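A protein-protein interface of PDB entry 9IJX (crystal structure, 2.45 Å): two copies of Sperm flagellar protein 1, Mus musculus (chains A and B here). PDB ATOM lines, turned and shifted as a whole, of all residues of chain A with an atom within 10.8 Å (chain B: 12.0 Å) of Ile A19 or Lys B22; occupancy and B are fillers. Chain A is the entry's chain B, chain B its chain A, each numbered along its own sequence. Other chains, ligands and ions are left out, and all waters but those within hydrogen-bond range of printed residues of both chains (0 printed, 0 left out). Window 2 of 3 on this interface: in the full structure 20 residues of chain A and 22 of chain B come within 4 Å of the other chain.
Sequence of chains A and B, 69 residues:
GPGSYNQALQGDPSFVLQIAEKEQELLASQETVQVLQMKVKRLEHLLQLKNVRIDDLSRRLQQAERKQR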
ATOM      1  N   LEU A  17      20.125  -6.354   3.925  1.00  0.00           N
ATOM      2  CA  LEU A  17      18.755  -6.181   4.454  1.00  0.00           C
ATOM      3  C   LEU A  17      18.536  -4.773   5.039  1.00  0.00           C
ATOM      4  O   LEU A  17      19.508  -4.046   5.309  1.00  0.00           O
ATOM      5  CB  LEU A  17      18.526  -7.250   5.528  1.00  0.00           C
ATOM      6  CG  LEU A  17      18.319  -8.670   5.006  1.00  0.00           C
ATOM      7  CD1 LEU A  17      18.390  -9.676   6.144  1.00  0.00           C
ATOM      8  CD2 LEU A  17      16.992  -8.790   4.274  1.00  0.00           C
ATOM      9  N   GLN A  18      17.268  -4.450   5.293  1.00  0.00           N
ATOM     10  CA  GLN A  18      16.787  -3.395   6.227  1.00  0.00           C
ATOM     11  C   GLN A  18      17.567  -3.470   7.550  1.00  0.00           C
ATOM     12  O   GLN A  18      17.978  -2.414   8.026  1.00  0.00           O
ATOM     13  CB  GLN A  18      15.275  -3.568   6.463  1.00  0.00           C
ATOM     14  CG  GLN A  18      14.395  -3.262   5.256  1.00  0.00           C
ATOM     15  CD  GLN A  18      14.329  -4.399   4.260  1.00  0.00           C
ATOM     16  OE1 GLN A  18      14.240  -5.571   4.622  1.00  0.00           O
ATOM     17  NE2 GLN A  18      14.395  -4.061   2.982  1.00  0.00           N
ATOM     18  N   ILE A  19      17.728  -4.674   8.115  1.00  0.00           N
ATOM     19  CA  ILE A  19      18.377  -4.955   9.424  1.00  0.00           C
ATOM     20  C   ILE A  19      19.871  -4.627   9.354  1.00  0.00           C
ATOM     21  O   ILE A  19      20.362  -4.049  10.335  1.00  0.00           O
ATOM     22  CB  ILE A  19      18.127  -6.428   9.841  1.00  0.00           C
ATOM     23  CG1 ILE A  19      16.633  -6.751   9.969  1.00  0.00           C
ATOM     24  CG2 ILE A  19      18.887  -6.791  11.114  1.00  0.00           C
ATOM     25  CD1 ILE A  19      16.135  -7.806   8.999  1.00  0.00           C
ATOM     26  N   ALA A  20      20.555  -4.958   8.254  1.00  0.00           N
ATOM     27  CA  ALA A  20      21.974  -4.613   7.997  1.00  0.00           C
ATOM     28  C   ALA A  20      22.182  -3.093   8.080  1.00  0.00           C
ATOM     29  O   ALA A  20      23.218  -2.654   8.646  1.00  0.00           O
ATOM     30  CB  ALA A  20      22.416  -5.150   6.662  1.00  0.00           C
ATOM     31  N   GLU A  21      21.233  -2.325   7.533  1.00  0.00           N
ATOM     32  CA  GLU A  21      21.280  -0.836   7.505  1.00  0.00           C
ATOM     33  C   GLU A  21      21.092  -0.308   8.934  1.00  0.00           C
ATOM     34  O   GLU A  21      21.903   0.542   9.361  1.00  0.00           O
ATOM     35  CB  GLU A  21      20.236  -0.286   6.522  1.00  0.00           C
ATOM     36  CG  GLU A  21      19.064   0.463   7.160  1.00  0.00           C
ATOM     37  CD  GLU A  21      17.779   0.419   6.347  1.00  0.00           C
ATOM     38  OE1 GLU A  21      17.887   0.348   5.104  1.00  0.00           O
ATOM     39  OE2 GLU A  21      16.681   0.425   6.961  1.00  0.00           O
ATOM     40  N   LYS A  22      20.076  -0.818   9.642  1.00  0.00           N
ATOM     41  CA  LYS A  22      19.708  -0.410  11.026  1.00  0.00           C
ATOM     42  C   LYS A  22      20.857  -0.740  11.983  1.00  0.00           C
ATOM     43  O   LYS A  22      21.080   0.046  12.895  1.00  0.00           O
ATOM     44  CB  LYS A  22      18.426  -1.114  11.495  1.00  0.00           C
ATOM     45  CG  LYS A  22      17.120  -0.602  10.896  1.00  0.00           C
ATOM     46  CD  LYS A  22      16.857   0.872  11.130  1.00  0.00           C
ATOM     47  N   GLU A  23      21.529  -1.875  11.781  1.00  0.00           N
ATOM     48  CA  GLU A  23      22.655  -2.340  12.634  1.00  0.00           C
ATOM     49  C   GLU A  23      23.877  -1.453  12.376  1.00  0.00           C
ATOM     50  O   GLU A  23      24.647  -1.248  13.335  1.00  0.00           O
ATOM     51  CB  GLU A  23      22.955  -3.819  12.374  1.00  0.00           C
ATOM     52  CG  GLU A  23      23.795  -4.471  13.451  1.00  0.00           C
ATOM     53  CD  GLU A  23      23.315  -4.252  14.876  1.00  0.00           C
ATOM     54  OE1 GLU A  23      22.107  -4.461  15.150  1.00  0.00           O
ATOM     55  OE2 GLU A  23      24.155  -3.865  15.707  1.00  0.00           O
ATOM     56  N   GLN A  24      24.037  -0.929  11.152  1.00  0.00           N
ATOM     57  CA  GLN A  24      25.192  -0.072  10.766  1.00  0.00           C
ATOM     58  C   GLN A  24      24.995   1.346  11.336  1.00  0.00           C
ATOM     59  O   GLN A  24      26.021   1.990  11.764  1.00  0.00           O
ATOM     60  CB  GLN A  24      25.421  -0.134   9.252  1.00  0.00           C
ATOM     61  CG  GLN A  24      24.508   0.679   8.336  1.00  0.00           C
ATOM     62  CD  GLN A  24      24.714   0.356   6.878  1.00  0.00           C
ATOM     63  OE1 GLN A  24      25.778  -0.089   6.444  1.00  0.00           O
ATOM     64  NE2 GLN A  24      23.679   0.592   6.092  1.00  0.00           N
ATOM     65  N   GLU A  25      23.738   1.811  11.346  1.00  0.00           N
ATOM     66  CA  GLU A  25      23.335   3.110  11.953  1.00  0.00           C
ATOM     67  C   GLU A  25      23.620   3.071  13.463  1.00  0.00           C
ATOM     68  O   GLU A  25      24.145   4.063  13.995  1.00  0.00           O
ATOM     69  CB  GLU A  25      21.855   3.399  11.670  1.00  0.00           C
ATOM     70  CG  GLU A  25      21.563   3.752  10.216  1.00  0.00           C
ATOM     71  CD  GLU A  25      20.104   3.680   9.776  1.00  0.00           C
ATOM     72  OE1 GLU A  25      19.242   3.358  10.617  1.00  0.00           O
ATOM     73  OE2 GLU A  25      19.837   3.886   8.573  1.00  0.00           O
ATOM     74  N   LEU A  26      23.280   1.953  14.114  1.00  0.00           N
ATOM     75  CA  LEU A  26      23.438   1.726  15.579  1.00  0.00           C
ATOM     76  C   LEU A  26      24.922   1.653  15.931  1.00  0.00           C
ATOM     77  O   LEU A  26      25.286   2.230  16.946  1.00  0.00           O
ATOM     78  CB  LEU A  26      22.690   0.441  15.968  1.00  0.00           C
ATOM     79  CG  LEU A  26      23.066  -0.207  17.298  1.00  0.00           C
ATOM     80  CD1 LEU A  26      21.891  -0.938  17.937  1.00  0.00           C
ATOM     81  CD2 LEU A  26      24.237  -1.154  17.064  1.00  0.00           C
ATOM     82  N   LEU A  27      25.736   0.953  15.144  1.00  0.00           N
ATOM     83  CA  LEU A  27      27.199   0.801  15.377  1.00  0.00           C
ATOM     84  C   LEU A  27      27.849   2.191  15.414  1.00  0.00           C
ATOM     85  O   LEU A  27      28.609   2.468  16.377  1.00  0.00           O
ATOM     86  CB  LEU A  27      27.799  -0.068  14.271  1.00  0.00           C
ATOM     87  CG  LEU A  27      27.413  -1.544  14.310  1.00  0.00           C
ATOM     88  CD1 LEU A  27      27.990  -2.289  13.114  1.00  0.00           C
ATOM     89  CD2 LEU A  27      27.842  -2.203  15.613  1.00  0.00           C
ATOM     90  N   SER A  29      26.423   5.078  16.025  1.00  0.00           N
ATOM     91  CA  SER A  29      25.884   5.723  17.254  1.00  0.00           C
ATOM     92  C   SER A  29      26.641   5.204  18.478  1.00  0.00           C
ATOM     93  O   SER A  29      27.092   6.024  19.264  1.00  0.00           O
ATOM     94  CB  SER A  29      24.393   5.499  17.398  1.00  0.00           C
ATOM     95  OG  SER A  29      23.662   6.292  16.476  1.00  0.00           O
ATOM     96  N   GLN A  30      26.787   3.887  18.615  1.00  0.00           N
ATOM     97  CA  GLN A  30      27.443   3.216  19.773  1.00  0.00           C
ATOM     98  C   GLN A  30      28.906   3.650  19.874  1.00  0.00           C
ATOM     99  O   GLN A  30      29.410   3.668  21.002  1.00  0.00           O
ATOM    100  CB  GLN A  30      27.320   1.693  19.657  1.00  0.00           C
ATOM    101  CG  GLN A  30      25.924   1.190  20.012  1.00  0.00           C
ATOM    102  CD  GLN A  30      25.792  -0.304  19.870  1.00  0.00           C
ATOM    103  OE1 GLN A  30      26.640  -0.970  19.280  1.00  0.00           O
ATOM    104  NE2 GLN A  30      24.715  -0.840  20.429  1.00  0.00           N
ATOM    105  N   GLY B  11       5.593 -15.701  10.209  1.00  0.00           N
ATOM    106  CA  GLY B  11       6.430 -15.413   9.004  1.00  0.00           C
ATOM    107  C   GLY B  11       6.819 -13.947   8.926  1.00  0.00           C
ATOM    108  O   GLY B  11       7.768 -13.557   9.624  1.00  0.00           O
ATOM    109  N   ASP B  12       6.102 -13.167   8.109  1.00  0.00           N
ATOM    110  CA  ASP B  12       6.309 -11.703   7.934  1.00  0.00           C
ATOM    111  C   ASP B  12       6.122 -10.977   9.265  1.00  0.00           C
ATOM    112  O   ASP B  12       6.927 -10.119   9.596  1.00  0.00           O
ATOM    113  CB  ASP B  12       5.425 -11.142   6.818  1.00  0.00           C
ATOM    114  CG  ASP B  12       5.511  -9.633   6.654  1.00  0.00           C
ATOM    115  OD1 ASP B  12       6.605  -9.135   6.298  1.00  0.00           O
ATOM    116  OD2 ASP B  12       4.483  -8.970   6.883  1.00  0.00           O
ATOM    117  N   PRO B  13       5.136 -11.329  10.124  1.00  0.00           N
ATOM    118  CA  PRO B  13       5.057 -10.796  11.488  1.00  0.00           C
ATOM    119  C   PRO B  13       6.325 -10.930  12.349  1.00  0.00           C
ATOM    120  O   PRO B  13       6.552 -10.054  13.165  1.00  0.00           O
ATOM    121  CB  PRO B  13       3.942 -11.630  12.129  1.00  0.00           C
ATOM    122  CG  PRO B  13       3.039 -11.951  10.967  1.00  0.00           C
ATOM    123  CD  PRO B  13       3.997 -12.207   9.822  1.00  0.00           C
ATOM    124  N   SER B  14       7.125 -11.983  12.161  1.00  0.00           N
ATOM    125  CA  SER B  14       8.430 -12.148  12.864  1.00  0.00           C
ATOM    126  C   SER B  14       9.367 -11.013  12.438  1.00  0.00           C
ATOM    127  O   SER B  14      10.114 -10.483  13.285  1.00  0.00           O
ATOM    128  CB  SER B  14       9.060 -13.504  12.618  1.00  0.00           C
ATOM    129  OG  SER B  14       9.956 -13.479  11.513  1.00  0.00           O
ATOM    130  N   PHE B  15       9.300 -10.648  11.156  1.00  0.00           N
ATOM    131  CA  PHE B  15      10.193  -9.668  10.489  1.00  0.00           C
ATOM    132  C   PHE B  15       9.786  -8.260  10.917  1.00  0.00           C
ATOM    133  O   PHE B  15      10.673  -7.486  11.212  1.00  0.00           O
ATOM    134  CB  PHE B  15      10.185  -9.909   8.975  1.00  0.00           C
ATOM    135  CG  PHE B  15      10.760 -11.250   8.589  1.00  0.00           C
ATOM    136  CD1 PHE B  15      12.029 -11.617   9.029  1.00  0.00           C
ATOM    137  CD2 PHE B  15      10.049 -12.152   7.800  1.00  0.00           C
ATOM    138  CE1 PHE B  15      12.572 -12.850   8.696  1.00  0.00           C
ATOM    139  CE2 PHE B  15      10.597 -13.382   7.465  1.00  0.00           C
ATOM    140  CZ  PHE B  15      11.858 -13.727   7.910  1.00  0.00           C
ATOM    141  N   VAL B  16       8.484  -7.976  10.973  1.00  0.00           N
ATOM    142  CA  VAL B  16       7.880  -6.725  11.533  1.00  0.00           C
ATOM    143  C   VAL B  16       8.425  -6.492  12.955  1.00  0.00           C
ATOM    144  O   VAL B  16       8.709  -5.332  13.302  1.00  0.00           O
ATOM    145  CB  VAL B  16       6.334  -6.832  11.511  1.00  0.00           C
ATOM    146  CG1 VAL B  16       5.625  -5.858  12.445  1.00  0.00           C
ATOM    147  CG2 VAL B  16       5.777  -6.712  10.098  1.00  0.00           C
ATOM    148  N   LEU B  17       8.538  -7.561  13.753  1.00  0.00           N
ATOM    149  CA  LEU B  17       8.963  -7.513  15.178  1.00  0.00           C
ATOM    150  C   LEU B  17      10.478  -7.317  15.246  1.00  0.00           C
ATOM    151  O   LEU B  17      10.934  -6.485  16.064  1.00  0.00           O
ATOM    152  CB  LEU B  17       8.546  -8.811  15.875  1.00  0.00           C
ATOM    153  CG  LEU B  17       7.042  -9.010  16.051  1.00  0.00           C
ATOM    154  CD1 LEU B  17       6.705 -10.458  16.382  1.00  0.00           C
ATOM    155  CD2 LEU B  17       6.504  -8.060  17.113  1.00  0.00           C
ATOM    156  N   GLN B  18      11.218  -8.085  14.441  1.00  0.00           N
ATOM    157  CA  GLN B  18      12.702  -8.016  14.323  1.00  0.00           C
ATOM    158  C   GLN B  18      13.131  -6.566  14.027  1.00  0.00           C
ATOM    159  O   GLN B  18      14.054  -6.080  14.711  1.00  0.00           O
ATOM    160  CB  GLN B  18      13.179  -8.980  13.238  1.00  0.00           C
ATOM    161  CG  GLN B  18      14.686  -8.965  13.007  1.00  0.00           C
ATOM    162  CD  GLN B  18      15.412 -10.001  13.825  1.00  0.00           C
ATOM    163  OE1 GLN B  18      14.974 -11.147  13.934  1.00  0.00           O
ATOM    164  NE2 GLN B  18      16.568  -9.619  14.355  1.00  0.00           N
ATOM    165  N   ILE B  19      12.489  -5.908  13.052  1.00  0.00           N
ATOM    166  CA  ILE B  19      12.866  -4.537  12.582  1.00  0.00           C
ATOM    167  C   ILE B  19      12.439  -3.519  13.641  1.00  0.00           C
ATOM    168  O   ILE B  19      13.219  -2.573  13.885  1.00  0.00           O
ATOM    169  CB  ILE B  19      12.262  -4.215  11.199  1.00  0.00           C
ATOM    170  N   ALA B  20      11.276  -3.720  14.272  1.00  0.00           N
ATOM    171  CA  ALA B  20      10.773  -2.916  15.413  1.00  0.00           C
ATOM    172  C   ALA B  20      11.792  -2.941  16.559  1.00  0.00           C
ATOM    173  O   ALA B  20      11.983  -1.886  17.190  1.00  0.00           O
ATOM    174  CB  ALA B  20       9.431  -3.444  15.866  1.00  0.00           C
ATOM    175  N   GLU B  21      12.407  -4.103  16.815  1.00  0.00           N
ATOM    176  CA  GLU B  21      13.419  -4.304  17.889  1.00  0.00           C
ATOM    177  C   GLU B  21      14.691  -3.520  17.532  1.00  0.00           C
ATOM    178  O   GLU B  21      15.184  -2.782  18.397  1.00  0.00           O
ATOM    179  CB  GLU B  21      13.670  -5.800  18.101  1.00  0.00           C
ATOM    180  CG  GLU B  21      15.109  -6.233  17.910  1.00  0.00           C
ATOM    181  CD  GLU B  21      15.383  -7.677  18.287  1.00  0.00           C
ATOM    182  OE1 GLU B  21      14.513  -8.329  18.929  1.00  0.00           O
ATOM    183  OE2 GLU B  21      16.485  -8.156  17.954  1.00  0.00           O
ATOM    184  N   LYS B  22      15.185  -3.684  16.302  1.00  0.00           N
ATOM    185  CA  LYS B  22      16.435  -3.051  15.791  1.00  0.00           C
ATOM    186  C   LYS B  22      16.269  -1.523  15.788  1.00  0.00           C
ATOM    187  O   LYS B  22      17.261  -0.812  16.100  1.00  0.00           O
ATOM    188  CB  LYS B  22      16.770  -3.504  14.368  1.00  0.00           C
ATOM    189  CG  LYS B  22      17.272  -4.928  14.184  1.00  0.00           C
ATOM    190  CD  LYS B  22      18.450  -5.370  15.023  1.00  0.00           C
ATOM    191  CE  LYS B  22      18.613  -6.880  14.968  1.00  0.00           C
ATOM    192  NZ  LYS B  22      20.005  -7.317  15.227  1.00  0.00           N
ATOM    193  N   GLU B  23      15.071  -1.033  15.446  1.00  0.00           N
ATOM    194  CA  GLU B  23      14.763   0.419  15.375  1.00  0.00           C
ATOM    195  C   GLU B  23      14.702   0.988  16.799  1.00  0.00           C
ATOM    196  O   GLU B  23      15.067   2.167  16.979  1.00  0.00           O
ATOM    197  CB  GLU B  23      13.473   0.668  14.590  1.00  0.00           C
ATOM    198  CG  GLU B  23      13.661   0.512  13.090  1.00  0.00           C
ATOM    199  CD  GLU B  23      12.480   0.912  12.224  1.00  0.00           C
ATOM    200  OE1 GLU B  23      11.341   0.470  12.507  1.00  0.00           O
ATOM    201  OE2 GLU B  23      12.705   1.659  11.256  1.00  0.00           O
ATOM    202  N   GLN B  24      14.274   0.181  17.771  1.00  0.00           N
ATOM    203  CA  GLN B  24      14.123   0.605  19.191  1.00  0.00           C
ATOM    204  C   GLN B  24      15.497   0.620  19.870  1.00  0.00           C
ATOM    205  O   GLN B  24      15.709   1.479  20.730  1.00  0.00           O
ATOM    206  CB  GLN B  24      13.124  -0.302  19.913  1.00  0.00           C
ATOM    207  CG  GLN B  24      12.627   0.286  21.222  1.00  0.00           C
ATOM    208  CD  GLN B  24      11.118   0.319  21.303  1.00  0.00           C
ATOM    209  OE1 GLN B  24      10.410   0.410  20.296  1.00  0.00           O
ATOM    210  NE2 GLN B  24      10.603   0.258  22.521  1.00  0.00           N
ATOM    211  N   GLU B  25      16.392  -0.295  19.488  1.00  0.00           N
ATOM    212  CA  GLU B  25      17.809  -0.342  19.947  1.00  0.00           C
ATOM    213  C   GLU B  25      18.529   0.925  19.469  1.00  0.00           C
ATOM    214  O   GLU B  25      19.275   1.516  20.281  1.00  0.00           O
ATOM    215  CB  GLU B  25      18.508  -1.607  19.437  1.00  0.00           C
ATOM    216  CG  GLU B  25      18.029  -2.885  20.120  1.00  0.00           C
ATOM    217  CD  GLU B  25      18.510  -4.191  19.505  1.00  0.00           C
ATOM    218  OE1 GLU B  25      19.496  -4.151  18.728  1.00  0.00           O
ATOM    219  OE2 GLU B  25      17.958  -5.267  19.856  1.00  0.00           O
ATOM    220  N   LEU B  26      18.296   1.328  18.214  1.00  0.00           N
ATOM    221  CA  LEU B  26      18.919   2.521  17.581  1.00  0.00           C
ATOM    222  C   LEU B  26      18.412   3.805  18.263  1.00  0.00           C
ATOM    223  O   LEU B  26      19.235   4.713  18.547  1.00  0.00           O
ATOM    224  CB  LEU B  26      18.609   2.541  16.079  1.00  0.00           C
ATOM    225  CG  LEU B  26      19.094   3.814  15.378  1.00  0.00           C
ATOM    226  CD1 LEU B  26      20.617   3.819  15.272  1.00  0.00           C
ATOM    227  CD2 LEU B  26      18.469   3.984  14.003  1.00  0.00           C
ATOM    228  N   LEU B  27      17.098   3.889  18.489  1.00  0.00           N
ATOM    229  CA  LEU B  27      16.436   5.053  19.137  1.00  0.00           C
ATOM    230  C   LEU B  27      17.066   5.286  20.513  1.00  0.00           C
ATOM    231  O   LEU B  27      17.428   6.435  20.805  1.00  0.00           O
ATOM    232  CB  LEU B  27      14.931   4.782  19.257  1.00  0.00           C
ATOM    233  CG  LEU B  27      14.078   5.169  18.049  1.00  0.00           C
ATOM    234  CD1 LEU B  27      12.626   4.767  18.267  1.00  0.00           C
ATOM    235  CD2 LEU B  27      14.189   6.660  17.763  1.00  0.00           C
ATOM    236  N   ALA B  28      17.192   4.226  21.317  1.00  0.00           N
ATOM    237  CA  ALA B  28      17.791   4.228  22.674  1.00  0.00           C
ATOM    238  C   ALA B  28      19.224   4.759  22.613  1.00  0.00           C
ATOM    239  O   ALA B  28      19.581   5.536  23.502  1.00  0.00           O
ATOM    240  CB  ALA B  28      17.752   2.833  23.262  1.00  0.00           C
ATOM    241  N   SER B  29      20.007   4.348  21.614  1.00  0.00           N
ATOM    242  CA  SER B  29      21.401   4.807  21.371  1.00  0.00           C
ATOM    243  C   SER B  29      21.396   6.303  21.017  1.00  0.00           C
ATOM    244  O   SER B  29      22.171   7.074  21.655  1.00  0.00           O
ATOM    245  CB  SER B  29      22.064   3.983  20.297  1.00  0.00           C
ATOM    246  OG  SER B  29      23.477   4.131  20.327  1.00  0.00           O
ATOM    247  N   GLN B  30      20.539   6.702  20.069  1.00  0.00           N
ATOM    248  CA  GLN B  30      20.450   8.101  19.567  1.00  0.00           C
ATOM    249  C   GLN B  30      20.066   9.051  20.717  1.00  0.00           C
ATOM    250  O   GLN B  30      20.499  10.250  20.706  1.00  0.00           O
ATOM    251  CB  GLN B  30      19.454   8.195  18.412  1.00  0.00           C
ATOM    252  CG  GLN B  30      19.967   7.603  17.105  1.00  0.00           C
ATOM    253  CD  GLN B  30      18.922   7.602  16.012  1.00  0.00           C
ATOM    254  OE1 GLN B  30      17.746   7.879  16.251  1.00  0.00           O
ATOM    255  NE2 GLN B  30      19.351   7.319  14.792  1.00  0.00           N
ATOM    256  N   GLU B  31      19.286   8.563  21.688  1.00  0.00           N
ATOM    257  CA  GLU B  31      18.920   9.359  22.885  1.00  0.00           C
ATOM    258  C   GLU B  31      20.061   9.326  23.896  1.00  0.00           C
ATOM    259  O   GLU B  31      20.276  10.348  24.504  1.00  0.00           O
ATOM    260  CB  GLU B  31      17.598   8.926  23.504  1.00  0.00           C
ATOM    261  CG  GLU B  31      17.407   7.475  23.806  1.00  0.00           C
ATOM    262  CD  GLU B  31      15.912   7.220  23.860  1.00  0.00           C
ATOM    263  OE1 GLU B  31      15.410   6.503  22.980  1.00  0.00           O
ATOM    264  OE2 GLU B  31      15.249   7.826  24.729  1.00  0.00           O
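Of the 21 printed residues of chain B, 6 touch a printed residue of chain A.
Along chain B the printed residues that touch a printed residue of chain A span positions 22 to 30.
Among the printed residues, 9 pairs touch across the chains.
The side-chain amino group (NZ) of Lys B22 lies within salt-bridge range of the side-chain carboxylate (OE1) of Glu A23, 3.5 Å away.
Lys B22 touches Ile A19 (CE to CG2, 3.9 Å).
Glu B23 touches Lys A22 (CG to CD, 3.8 Å).
Leu B26 touches Glu A25.
CB of Glu B25 touches CD1 of Leu A26, at 3.8 Å.
Leu B26 touches Leu A26.
Ser A29 touches Ser B29 (CB to OG, 3.4 Å).
Ser A29 touches Gln B30 (OG to CG, 3.97 Å).
Gln A30 touches Ser B29.
Ile A19 touches Lys B22, but with the chains exchanged Lys A22 does not touch Ile B19 (5.3 Å).
Lys A22 touches Glu B23, and with the chains exchanged Glu A23 touches Lys B22.
Glu A25 touches Leu B26, and with the chains exchanged Leu A26 touches Glu B25.
Leu A26 touches its own counterpart, Leu B26.
Of chain B, only Lys B22 (3.9 Å) comes within 4 Å of Ile A19.
Lys B22 touches just these residues of chain A: Ile A19 and Glu A23.
No residue of chain B comes within 4 Å of Leu A17.
No residue of chain B comes within 4 Å of Gln A18.
No residue of chain B comes within 4 Å of Glu A21.
Glu A23 touches just one residue of chain B: Lys B22 (3.5 Å).
No residue of chain A comes within 4 Å of Gln B18.
No residue of chain A comes within 4 Å of Ala B20.
No residue of chain A comes within 4 Å of Glu B21.
Of chain A, only Lys A22 comes within 4 Å of Glu B23.
Of chain A, only Leu A26 comes within 4 Å of Glu B25.
Leu B26 touches two residues of chain A.
Printed residues of chain B within 4 Å of Gln A30: Ser B29 (3.7 Å).
Of the printed residues of chain B, Leu A26 touches Glu B25 and Leu B26.
Of the printed residues of chain A, Ser B29 touches Ser A29 and Gln A30.
Ser B14 touches none of the printed residues of chain A.
Leu B17 touches none of the printed residues of chain A.
O of Glu A25 lies within hydrogen-bond range of OG of Ser A29, at 3.4 Å.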
